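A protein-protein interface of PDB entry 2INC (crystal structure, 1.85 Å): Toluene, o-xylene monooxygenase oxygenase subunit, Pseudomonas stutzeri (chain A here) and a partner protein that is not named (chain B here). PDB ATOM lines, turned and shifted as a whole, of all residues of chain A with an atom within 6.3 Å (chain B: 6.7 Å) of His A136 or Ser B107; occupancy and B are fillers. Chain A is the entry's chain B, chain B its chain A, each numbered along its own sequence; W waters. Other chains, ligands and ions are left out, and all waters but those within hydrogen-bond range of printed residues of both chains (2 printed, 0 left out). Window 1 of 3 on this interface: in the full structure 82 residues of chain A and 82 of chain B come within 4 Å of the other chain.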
ATOM      1  N   HIS A  29       9.098 -22.792   8.520  1.00  0.00           N
ATOM      2  CA  HIS A  29       8.348 -22.350   7.349  1.00  0.00           C
ATOM      3  C   HIS A  29       6.894 -22.632   7.640  1.00  0.00           C
ATOM      4  O   HIS A  29       6.558 -23.705   8.165  1.00  0.00           O
ATOM      5  CB  HIS A  29       8.755 -23.079   6.077  1.00  0.00           C
ATOM      6  CG  HIS A  29      10.122 -22.697   5.601  1.00  0.00           C
ATOM      7  ND1 HIS A  29      10.893 -23.501   4.788  1.00  0.00           N
ATOM      8  CD2 HIS A  29      10.835 -21.567   5.797  1.00  0.00           C
ATOM      9  CE1 HIS A  29      12.041 -22.904   4.545  1.00  0.00           C
ATOM     10  NE2 HIS A  29      12.026 -21.717   5.129  1.00  0.00           N
ATOM     11  N   GLY A 131      22.807 -19.239  -7.051  1.00  0.00           N
ATOM     12  CA  GLY A 131      22.309 -20.639  -7.054  1.00  0.00           C
ATOM     13  C   GLY A 131      21.868 -21.100  -5.704  1.00  0.00           C
ATOM     14  O   GLY A 131      20.735 -21.578  -5.526  1.00  0.00           O
ATOM     15  N   SER A 132      22.739 -20.954  -4.717  1.00  0.00           N
ATOM     16  CA  SER A 132      22.397 -21.409  -3.382  1.00  0.00           C
ATOM     17  C   SER A 132      21.344 -20.553  -2.669  1.00  0.00           C
ATOM     18  O   SER A 132      20.580 -21.070  -1.823  1.00  0.00           O
ATOM     19  CB  SER A 132      23.671 -21.582  -2.502  1.00  0.00           C
ATOM     20  OG  SER A 132      24.304 -20.313  -2.362  1.00  0.00           O
ATOM     21  N   VAL A 133      21.226 -19.269  -3.037  1.00  0.00           N
ATOM     22  CA  VAL A 133      20.235 -18.433  -2.380  1.00  0.00           C
ATOM     23  C   VAL A 133      18.862 -18.694  -3.039  1.00  0.00           C
ATOM     24  O   VAL A 133      17.817 -18.433  -2.436  1.00  0.00           O
ATOM     25  CB  VAL A 133      20.621 -16.905  -2.414  1.00  0.00           C
ATOM     26  CG1 VAL A 133      20.215 -16.286  -3.663  1.00  0.00           C
ATOM     27  CG2 VAL A 133      20.102 -16.157  -1.151  1.00  0.00           C
ATOM     28  N   TYR A 134      18.871 -19.215  -4.264  1.00  0.00           N
ATOM     29  CA  TYR A 134      17.603 -19.735  -4.808  1.00  0.00           C
ATOM     30  C   TYR A 134      17.164 -20.994  -4.072  1.00  0.00           C
ATOM     31  O   TYR A 134      15.988 -21.082  -3.650  1.00  0.00           O
ATOM     32  CB  TYR A 134      17.590 -19.878  -6.331  1.00  0.00           C
ATOM     33  CG  TYR A 134      16.258 -20.440  -6.751  1.00  0.00           C
ATOM     34  CD1 TYR A 134      16.132 -21.810  -7.099  1.00  0.00           C
ATOM     35  CD2 TYR A 134      15.111 -19.669  -6.668  1.00  0.00           C
ATOM     36  CE1 TYR A 134      14.879 -22.340  -7.438  1.00  0.00           C
ATOM     37  CE2 TYR A 134      13.822 -20.221  -7.002  1.00  0.00           C
ATOM     38  CZ  TYR A 134      13.756 -21.541  -7.376  1.00  0.00           C
ATOM     39  OH  TYR A 134      12.495 -22.066  -7.684  1.00  0.00           O
ATOM     40  N   ILE A 135      18.078 -21.914  -3.799  1.00  0.00           N
ATOM     41  CA  ILE A 135      17.694 -23.119  -2.979  1.00  0.00           C
ATOM     42  C   ILE A 135      17.066 -22.694  -1.647  1.00  0.00           C
ATOM     43  O   ILE A 135      16.027 -23.235  -1.219  1.00  0.00           O
ATOM     44  CB  ILE A 135      18.896 -24.067  -2.795  1.00  0.00           C
ATOM     45  CG1 ILE A 135      19.301 -24.557  -4.194  1.00  0.00           C
ATOM     46  CG2 ILE A 135      18.615 -25.260  -1.780  1.00  0.00           C
ATOM     47  CD1 ILE A 135      20.673 -25.301  -4.367  1.00  0.00           C
ATOM     48  N   HIS A 136      17.703 -21.737  -0.981  1.00  0.00           N
ATOM     49  CA  HIS A 136      17.177 -21.169   0.263  1.00  0.00           C
ATOM     50  C   HIS A 136      15.683 -20.965   0.191  1.00  0.00           C
ATOM     51  O   HIS A 136      14.954 -21.415   1.070  1.00  0.00           O
ATOM     52  CB  HIS A 136      17.888 -19.830   0.549  1.00  0.00           C
ATOM     53  CG  HIS A 136      17.265 -19.032   1.647  1.00  0.00           C
ATOM     54  ND1 HIS A 136      17.947 -18.693   2.790  1.00  0.00           N
ATOM     55  CD2 HIS A 136      16.015 -18.530   1.789  1.00  0.00           C
ATOM     56  CE1 HIS A 136      17.154 -17.978   3.574  1.00  0.00           C
ATOM     57  NE2 HIS A 136      15.974 -17.875   2.991  1.00  0.00           N
ATOM     58  N   GLN A 137      15.223 -20.226  -0.819  1.00  0.00           N
ATOM     59  CA  GLN A 137      13.879 -19.676  -0.800  1.00  0.00           C
ATOM     60  C   GLN A 137      12.811 -20.692  -1.293  1.00  0.00           C
ATOM     61  O   GLN A 137      11.610 -20.482  -1.093  1.00  0.00           O
ATOM     62  CB  GLN A 137      13.844 -18.356  -1.589  1.00  0.00           C
ATOM     63  CG  GLN A 137      14.048 -18.498  -3.058  1.00  0.00           C
ATOM     64  CD  GLN A 137      14.494 -17.179  -3.694  1.00  0.00           C
ATOM     65  OE1 GLN A 137      15.691 -16.798  -3.688  1.00  0.00           O
ATOM     66  NE2 GLN A 137      13.580 -16.507  -4.238  1.00  0.00           N
ATOM     67  N   ILE A 138      13.227 -21.799  -1.901  1.00  0.00           N
ATOM     68  CA  ILE A 138      12.242 -22.800  -2.397  1.00  0.00           C
ATOM     69  C   ILE A 138      12.337 -24.150  -1.636  1.00  0.00           C
ATOM     70  O   ILE A 138      11.475 -25.021  -1.831  1.00  0.00           O
ATOM     71  CB  ILE A 138      12.456 -22.977  -3.924  1.00  0.00           C
ATOM     72  CG1 ILE A 138      11.262 -23.587  -4.692  1.00  0.00           C
ATOM     73  CG2 ILE A 138      13.765 -23.739  -4.193  1.00  0.00           C
ATOM     74  CD1 ILE A 138       9.935 -22.765  -4.644  1.00  0.00           C
ATOM     75  N   ALA A 139      13.332 -24.328  -0.777  1.00  0.00           N
ATOM     76  CA  ALA A 139      13.407 -25.602  -0.004  1.00  0.00           C
ATOM     77  C   ALA A 139      12.162 -25.787   0.879  1.00  0.00           C
ATOM     78  O   ALA A 139      11.612 -24.801   1.403  1.00  0.00           O
ATOM     79  CB  ALA A 139      14.660 -25.650   0.888  1.00  0.00           C
ATOM     80  N   ALA A 141      11.795 -27.149   4.065  1.00  0.00           N
ATOM     81  CA  ALA A 141      11.982 -27.244   5.506  1.00  0.00           C
ATOM     82  C   ALA A 141      12.997 -26.176   5.888  1.00  0.00           C
ATOM     83  O   ALA A 141      14.014 -26.000   5.186  1.00  0.00           O
ATOM     84  CB  ALA A 141      12.533 -28.549   5.872  1.00  0.00           C
ATOM     85  N   ILE A 144      16.631 -27.294   5.974  1.00  0.00           N
ATOM     86  CA  ILE A 144      17.251 -27.382   4.641  1.00  0.00           C
ATOM     87  C   ILE A 144      17.580 -25.943   4.204  1.00  0.00           C
ATOM     88  O   ILE A 144      18.711 -25.663   3.803  1.00  0.00           O
ATOM     89  CB  ILE A 144      16.321 -28.011   3.617  1.00  0.00           C
ATOM     90  CG1 ILE A 144      16.005 -29.451   3.999  1.00  0.00           C
ATOM     91  CG2 ILE A 144      16.962 -28.027   2.215  1.00  0.00           C
ATOM     92  CD1 ILE A 144      14.836 -30.011   3.107  1.00  0.00           C
ATOM     93  N   THR A 145      16.607 -25.045   4.281  1.00  0.00           N
ATOM     94  CA  THR A 145      16.877 -23.614   4.022  1.00  0.00           C
ATOM     95  C   THR A 145      18.116 -23.025   4.750  1.00  0.00           C
ATOM     96  O   THR A 145      18.920 -22.308   4.126  1.00  0.00           O
ATOM     97  CB  THR A 145      15.643 -22.738   4.338  1.00  0.00           C
ATOM     98  OG1 THR A 145      14.656 -22.985   3.356  1.00  0.00           O
ATOM     99  CG2 THR A 145      16.043 -21.249   4.338  1.00  0.00           C
ATOM    100  N   ASN A 146      18.297 -23.320   6.040  1.00  0.00           N
ATOM    101  CA  ASN A 146      19.417 -22.745   6.759  1.00  0.00           C
ATOM    102  C   ASN A 146      20.773 -23.231   6.240  1.00  0.00           C
ATOM    103  O   ASN A 146      21.691 -22.438   6.173  1.00  0.00           O
ATOM    104  CB  ASN A 146      19.322 -22.988   8.246  1.00  0.00           C
ATOM    105  CG  ASN A 146      18.225 -22.197   8.913  1.00  0.00           C
ATOM    106  OD1 ASN A 146      18.015 -22.354  10.112  1.00  0.00           O
ATOM    107  ND2 ASN A 146      17.509 -21.353   8.144  1.00  0.00           N
ATOM    108  N   ALA A 148      21.440 -23.842   3.172  1.00  0.00           N
ATOM    109  CA  ALA A 148      21.579 -22.999   1.950  1.00  0.00           C
ATOM    110  C   ALA A 148      21.919 -21.515   2.264  1.00  0.00           C
ATOM    111  O   ALA A 148      22.693 -20.850   1.504  1.00  0.00           O
ATOM    112  CB  ALA A 148      20.258 -23.116   1.042  1.00  0.00           C
ATOM    113  N   THR A 149      21.347 -20.994   3.362  1.00  0.00           N
ATOM    114  CA  THR A 149      21.670 -19.661   3.893  1.00  0.00           C
ATOM    115  C   THR A 149      23.162 -19.552   4.165  1.00  0.00           C
ATOM    116  O   THR A 149      23.797 -18.676   3.655  1.00  0.00           O
ATOM    117  CB  THR A 149      20.880 -19.333   5.226  1.00  0.00           C
ATOM    118  OG1 THR A 149      19.441 -19.465   4.982  1.00  0.00           O
ATOM    119  CG2 THR A 149      21.196 -17.830   5.682  1.00  0.00           C
ATOM    120  N   THR A 152      25.267 -19.850   1.054  1.00  0.00           N
ATOM    121  CA  THR A 152      25.216 -18.598   0.253  1.00  0.00           C
ATOM    122  C   THR A 152      26.248 -17.598   0.790  1.00  0.00           C
ATOM    123  O   THR A 152      26.960 -16.927   0.007  1.00  0.00           O
ATOM    124  CB  THR A 152      23.803 -17.994   0.257  1.00  0.00           C
ATOM    125  OG1 THR A 152      22.919 -18.972  -0.329  1.00  0.00           O
ATOM    126  CG2 THR A 152      23.749 -16.769  -0.618  1.00  0.00           C
ATOM    127  N   GLU B 102       8.051 -14.494  11.398  1.00  0.00           N
ATOM    128  CA  GLU B 102       8.057 -13.463  10.314  1.00  0.00           C
ATOM    129  C   GLU B 102       9.440 -12.832  10.085  1.00  0.00           C
ATOM    130  O   GLU B 102       9.797 -12.555   8.927  1.00  0.00           O
ATOM    131  CB  GLU B 102       6.999 -12.397  10.562  1.00  0.00           C
ATOM    132  CG  GLU B 102       5.510 -12.980  10.600  1.00  0.00           C
ATOM    133  CD  GLU B 102       5.019 -13.545   9.260  1.00  0.00           C
ATOM    134  OE1 GLU B 102       5.813 -13.799   8.314  1.00  0.00           O
ATOM    135  OE2 GLU B 102       3.794 -13.739   9.088  1.00  0.00           O
ATOM    136  N   GLU B 103      10.207 -12.627  11.157  1.00  0.00           N
ATOM    137  CA  GLU B 103      11.690 -12.319  10.999  1.00  0.00           C
ATOM    138  C   GLU B 103      12.354 -13.384  10.150  1.00  0.00           C
ATOM    139  O   GLU B 103      12.999 -13.092   9.131  1.00  0.00           O
ATOM    140  CB  GLU B 103      12.407 -12.271  12.348  1.00  0.00           C
ATOM    141  CG  GLU B 103      11.941 -11.142  13.286  1.00  0.00           C
ATOM    142  CD  GLU B 103      12.726  -9.847  13.091  1.00  0.00           C
ATOM    143  OE1 GLU B 103      13.275  -9.568  11.975  1.00  0.00           O
ATOM    144  OE2 GLU B 103      12.785  -9.077  14.064  1.00  0.00           O
ATOM    145  N   TYR B 104      12.165 -14.649  10.529  1.00  0.00           N
ATOM    146  CA  TYR B 104      12.746 -15.736   9.742  1.00  0.00           C
ATOM    147  C   TYR B 104      12.256 -15.781   8.289  1.00  0.00           C
ATOM    148  O   TYR B 104      13.068 -15.996   7.342  1.00  0.00           O
ATOM    149  CB  TYR B 104      12.547 -17.093  10.463  1.00  0.00           C
ATOM    150  CG  TYR B 104      13.208 -18.213   9.718  1.00  0.00           C
ATOM    151  CD1 TYR B 104      14.587 -18.410   9.800  1.00  0.00           C
ATOM    152  CD2 TYR B 104      12.433 -19.117   8.985  1.00  0.00           C
ATOM    153  CE1 TYR B 104      15.182 -19.469   9.098  1.00  0.00           C
ATOM    154  CE2 TYR B 104      12.999 -20.173   8.265  1.00  0.00           C
ATOM    155  CZ  TYR B 104      14.374 -20.346   8.337  1.00  0.00           C
ATOM    156  OH  TYR B 104      14.949 -21.373   7.611  1.00  0.00           O
ATOM    157  N   ALA B 105      10.966 -15.497   8.044  1.00  0.00           N
ATOM    158  CA  ALA B 105      10.455 -15.473   6.682  1.00  0.00           C
ATOM    159  C   ALA B 105      11.058 -14.303   5.896  1.00  0.00           C
ATOM    160  O   ALA B 105      11.208 -14.375   4.669  1.00  0.00           O
ATOM    161  CB  ALA B 105       8.861 -15.297   6.661  1.00  0.00           C
ATOM    162  N   ALA B 106      11.360 -13.220   6.593  1.00  0.00           N
ATOM    163  CA  ALA B 106      12.067 -12.103   5.970  1.00  0.00           C
ATOM    164  C   ALA B 106      13.421 -12.540   5.385  1.00  0.00           C
ATOM    165  O   ALA B 106      13.928 -11.912   4.432  1.00  0.00           O
ATOM    166  CB  ALA B 106      12.232 -10.989   6.964  1.00  0.00           C
ATOM    167  N   SER B 107      14.026 -13.626   5.889  1.00  0.00           N
ATOM    168  CA  SER B 107      15.275 -14.010   5.249  1.00  0.00           C
ATOM    169  C   SER B 107      14.950 -14.517   3.845  1.00  0.00           C
ATOM    170  O   SER B 107      15.780 -14.401   2.960  1.00  0.00           O
ATOM    171  CB  SER B 107      16.088 -15.029   6.040  1.00  0.00           C
ATOM    172  OG  SER B 107      15.363 -16.242   6.138  1.00  0.00           O
ATOM    173  N   THR B 108      13.757 -15.108   3.636  1.00  0.00           N
ATOM    174  CA  THR B 108      13.342 -15.533   2.277  1.00  0.00           C
ATOM    175  C   THR B 108      13.050 -14.344   1.394  1.00  0.00           C
ATOM    176  O   THR B 108      13.366 -14.339   0.206  1.00  0.00           O
ATOM    177  CB  THR B 108      12.147 -16.505   2.319  1.00  0.00           C
ATOM    178  OG1 THR B 108      12.616 -17.775   2.797  1.00  0.00           O
ATOM    179  CG2 THR B 108      11.487 -16.684   0.895  1.00  0.00           C
ATOM    180  N   ALA B 109      12.418 -13.331   1.970  1.00  0.00           N
ATOM    181  CA  ALA B 109      12.171 -12.113   1.221  1.00  0.00           C
ATOM    182  C   ALA B 109      13.536 -11.492   0.812  1.00  0.00           C
ATOM    183  O   ALA B 109      13.689 -11.008  -0.312  1.00  0.00           O
ATOM    184  CB  ALA B 109      11.400 -11.147   2.063  1.00  0.00           C
ATOM    185  N   GLU B 110      14.537 -11.563   1.694  1.00  0.00           N
ATOM    186  CA  GLU B 110      15.891 -11.041   1.314  1.00  0.00           C
ATOM    187  C   GLU B 110      16.482 -11.951   0.205  1.00  0.00           C
ATOM    188  O   GLU B 110      17.054 -11.468  -0.776  1.00  0.00           O
ATOM    189  CB  GLU B 110      16.773 -10.931   2.567  1.00  0.00           C
ATOM    190  CG  GLU B 110      16.306  -9.803   3.555  1.00  0.00           C
ATOM    191  CD  GLU B 110      16.751  -8.377   3.111  1.00  0.00           C
ATOM    192  OE1 GLU B 110      17.555  -8.283   2.158  1.00  0.00           O
ATOM    193  OE2 GLU B 110      16.323  -7.329   3.692  1.00  0.00           O
ATOM    194  N   ALA B 111      16.348 -13.284   0.385  1.00  0.00           N
ATOM    195  CA  ALA B 111      16.815 -14.247  -0.624  1.00  0.00           C
ATOM    196  C   ALA B 111      16.189 -13.975  -1.985  1.00  0.00           C
ATOM    197  O   ALA B 111      16.863 -14.097  -3.037  1.00  0.00           O
ATOM    198  CB  ALA B 111      16.503 -15.711  -0.135  1.00  0.00           C
ATOM    199  N   ARG B 112      14.904 -13.591  -2.020  1.00  0.00           N
ATOM    200  CA  ARG B 112      14.270 -13.168  -3.308  1.00  0.00           C
ATOM    201  C   ARG B 112      15.114 -12.107  -4.017  1.00  0.00           C
ATOM    202  O   ARG B 112      15.385 -12.225  -5.236  1.00  0.00           O
ATOM    203  CB  ARG B 112      12.832 -12.594  -3.101  1.00  0.00           C
ATOM    204  CG  ARG B 112      11.905 -12.693  -4.349  1.00  0.00           C
ATOM    205  CD  ARG B 112      11.360 -14.111  -4.584  1.00  0.00           C
ATOM    206  NE  ARG B 112      10.300 -14.377  -3.611  1.00  0.00           N
ATOM    207  CZ  ARG B 112      10.117 -15.538  -2.969  1.00  0.00           C
ATOM    208  NH1 ARG B 112      10.888 -16.583  -3.211  1.00  0.00           N
ATOM    209  NH2 ARG B 112       9.101 -15.680  -2.147  1.00  0.00           N
ATOM    210  N   ALA B 126      21.394  -7.878  -0.042  1.00  0.00           N
ATOM    211  CA  ALA B 126      20.290  -8.800   0.308  1.00  0.00           C
ATOM    212  C   ALA B 126      20.838 -10.096   0.857  1.00  0.00           C
ATOM    213  O   ALA B 126      20.185 -10.743   1.644  1.00  0.00           O
ATOM    214  CB  ALA B 126      19.376  -9.075  -0.889  1.00  0.00           C
ATOM    215  N   GLY B 129      21.354  -9.049   4.243  1.00  0.00           N
ATOM    216  CA  GLY B 129      19.972  -9.009   4.828  1.00  0.00           C
ATOM    217  C   GLY B 129      19.437 -10.392   5.156  1.00  0.00           C
ATOM    218  O   GLY B 129      18.786 -10.617   6.205  1.00  0.00           O
ATOM    219  N   MET B 130      19.662 -11.321   4.234  1.00  0.00           N
ATOM    220  CA  MET B 130      19.195 -12.697   4.456  1.00  0.00           C
ATOM    221  C   MET B 130      19.825 -13.240   5.720  1.00  0.00           C
ATOM    222  O   MET B 130      19.126 -13.775   6.603  1.00  0.00           O
ATOM    223  CB  MET B 130      19.549 -13.560   3.241  1.00  0.00           C
ATOM    224  CG  MET B 130      19.511 -15.017   3.583  1.00  0.00           C
ATOM    225  SD  MET B 130      20.391 -15.882   2.324  1.00  0.00           S
ATOM    226  CE  MET B 130      22.069 -15.575   2.904  1.00  0.00           C
ATOM    227  N   MET B 131      21.131 -13.048   5.880  1.00  0.00           N
ATOM    228  CA  MET B 131      21.824 -13.379   7.167  1.00  0.00           C
ATOM    229  C   MET B 131      21.284 -12.691   8.407  1.00  0.00           C
ATOM    230  O   MET B 131      21.112 -13.302   9.462  1.00  0.00           O
ATOM    231  CB  MET B 131      23.340 -13.124   7.060  1.00  0.00           C
ATOM    232  CG  MET B 131      24.012 -14.108   6.095  1.00  0.00           C
ATOM    233  SD  MET B 131      24.022 -15.792   6.917  1.00  0.00           S
ATOM    234  CE  MET B 131      25.372 -15.628   8.115  1.00  0.00           C
ATOM    235  N   ASP B 132      21.050 -11.405   8.302  1.00  0.00           N
ATOM    236  CA  ASP B 132      20.501 -10.648   9.443  1.00  0.00           C
ATOM    237  C   ASP B 132      19.149 -11.173   9.942  1.00  0.00           C
ATOM    238  O   ASP B 132      18.980 -11.369  11.133  1.00  0.00           O
ATOM    239  CB  ASP B 132      20.257  -9.186   9.043  1.00  0.00           C
ATOM    240  CG  ASP B 132      21.541  -8.395   8.865  1.00  0.00           C
ATOM    241  OD1 ASP B 132      22.598  -8.840   9.368  1.00  0.00           O
ATOM    242  OD2 ASP B 132      21.464  -7.323   8.200  1.00  0.00           O
ATOM    243  N   GLU B 133      18.211 -11.419   9.022  1.00  0.00           N
ATOM    244  CA  GLU B 133      16.894 -11.955   9.408  1.00  0.00           C
ATOM    245  C   GLU B 133      17.004 -13.373   9.920  1.00  0.00           C
ATOM    246  O   GLU B 133      16.236 -13.825  10.782  1.00  0.00           O
ATOM    247  CB  GLU B 133      15.945 -11.868   8.221  1.00  0.00           C
ATOM    248  CG  GLU B 133      15.846 -10.450   7.589  1.00  0.00           C
ATOM    249  CD  GLU B 133      15.299  -9.356   8.507  1.00  0.00           C
ATOM    250  OE1 GLU B 133      15.204  -9.563   9.706  1.00  0.00           O
ATOM    251  OE2 GLU B 133      14.956  -8.243   8.023  1.00  0.00           O
ATOM    252  N   ASN B 134      17.963 -14.116   9.395  1.00  0.00           N
ATOM    253  CA  ASN B 134      18.295 -15.416  10.012  1.00  0.00           C
ATOM    254  C   ASN B 134      18.652 -15.258  11.492  1.00  0.00           C
ATOM    255  O   ASN B 134      18.096 -15.942  12.367  1.00  0.00           O
ATOM    256  CB  ASN B 134      19.419 -16.060   9.201  1.00  0.00           C
ATOM    257  CG  ASN B 134      19.821 -17.419   9.770  1.00  0.00           C
ATOM    258  OD1 ASN B 134      20.704 -17.485  10.618  1.00  0.00           O
ATOM    259  ND2 ASN B 134      19.186 -18.498   9.295  1.00  0.00           N
ATOM    260  N   MET B 179       6.181  -8.890   1.428  1.00  0.00           N
ATOM    261  CA  MET B 179       7.514  -9.393   1.244  1.00  0.00           C
ATOM    262  C   MET B 179       7.657 -10.789   0.650  1.00  0.00           C
ATOM    263  O   MET B 179       8.721 -11.091   0.071  1.00  0.00           O
ATOM    264  CB  MET B 179       8.289  -9.275   2.554  1.00  0.00           C
ATOM    265  CG  MET B 179       8.074 -10.412   3.555  1.00  0.00           C
ATOM    266  SD  MET B 179       8.956 -10.025   5.094  1.00  0.00           S
ATOM    267  CE  MET B 179       8.598 -11.585   6.022  1.00  0.00           C
ATOM    268  N   MET B 180       6.608 -11.629   0.731  1.00  0.00           N
ATOM    269  CA  MET B 180       6.745 -13.041   0.299  1.00  0.00           C
ATOM    270  C   MET B 180       6.183 -13.323  -1.066  1.00  0.00           C
ATOM    271  O   MET B 180       6.493 -14.367  -1.650  1.00  0.00           O
ATOM    272  CB  MET B 180       6.131 -14.039   1.306  1.00  0.00           C
ATOM    273  CG  MET B 180       6.488 -13.825   2.747  1.00  0.00           C
ATOM    274  SD  MET B 180       8.283 -13.958   3.029  1.00  0.00           S
ATOM    275  CE  MET B 180       8.484 -15.753   3.045  1.00  0.00           C
HETATM  276  O   HOH W   1      17.737 -18.421   6.922  1.00  0.00           O
HETATM  277  O   HOH W   2      10.743 -19.824   1.919  1.00  0.00           O
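A ring nitrogen (NE2) of His A136 is in hydrogen-bond range of the backbone carbonyl oxygen (O) of Ser B107, at 3.5 Å.
OH of Tyr B104 lies within hydrogen-bond range of ND2 of Asn A146 (2.6 Å).
The side-chain amide oxygen (OE1) of Gln A137 lies close to the backbone carbonyl oxygen (O) of Ala B111.
The side-chain sulfur (SD) of Met B130 is in hydrogen-bond range of a ring nitrogen (ND1) of His A136 (3.8 Å).
The guanidinium group (NH1) of Arg B112 sits close to the side-chain amide nitrogen (NE2) of Gln A137, 2.9 Å away.
NE2 of His A136 lies within hydrogen-bond range of OG1 of Thr B108.
OG1 of Thr A152 sits at hydrogen-bond distance from N of Val A133 (3.2 Å).
The backbone carbonyl oxygen of Tyr B104 lies within hydrogen-bond range of the side-chain hydroxyl of Ser B107, 2.6 Å away.
The side-chain hydroxyl (OG) of Ser A132 sits at hydrogen-bond distance from the side-chain hydroxyl (OG1) of Thr A152 (2.8 Å).
The backbone carbonyl oxygen of Val A133 lies close to the side-chain amide oxygen of Gln A137 (3.0 Å).
O of Ala A148 sits at hydrogen-bond distance from OG1 of Thr A152 (2.6 Å).
The guanidinium group (NH2) of Arg B112 lies within hydrogen-bond range of the backbone carbonyl oxygen (O) of Met B180, 3.0 Å away.
His A29 touches Tyr B104.
CB of Ala B111 touches CG2 of Val A133, 3.8 Å away.
Val A133 touches Met B130.
Ala B111 touches His A136 (CB to CD2, 3.4 Å).
CB of Gln A137 touches CG2 of Thr B108, at 3.8 Å.
CG2 of Thr A145 touches OH of Tyr B104, at 3.5 Å.
Asn A146 touches Asn B134 (ND2 to ND2, 3.5 Å).
O of Thr A149 touches CE of Met B130, 3.6 Å away.
Thr A149 touches Met B131 (CG2 to SD, 3.7 Å).
Thr A152 touches Met B130 (CB to CE, 3.98 Å).
Ser B107 touches just one residue of chain A: His A136 (3.5 Å).
Printed residues of chain B within 4 Å of Thr A152: Met B130.
Of the printed residues of chain A, Ala B111 touches Val A133, His A136 and Gln A137.
Ile A144 touches none of the printed residues of chain B.
The nearest residue of chain B that does not touch His A136 is Tyr B104 (5.6 Å).
The nearest residue of chain A that does not touch Ser B107 is Thr A149 (5.3 Å).
The nearest printed residue of chain B that does not touch Thr A145 is Thr B108 (5.1 Å).
Of the 17 printed residues of chain A, 8 touch a printed residue of chain B.
Hydrophobic or aromatic side chains of chain A within 4 Å of the printed part of chain B: His A29, Val A133 and His A136.
Among the printed residues, no Asp or Glu carboxylate lies within 4 Å of a Lys or Arg side-chain nitrogen of the other chain.
Water W1 lies within hydrogen-bond range of the side-chain amide nitrogen (ND2) of Asn B134 (2.8 Å), the side-chain hydroxyl (OG1) of Thr A149 (2.8 Å), the side-chain amide nitrogen (ND2) of Asn A146 (3.2 Å) and the side-chain hydroxyl (OG) of Ser B107 (3.3 Å).
Water W2 bridges the side-chain hydroxyl (OG1) of Thr B108 (2.9 Å) and the backbone carbonyl oxygen (O) of Gln A137 (3.2 Å).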
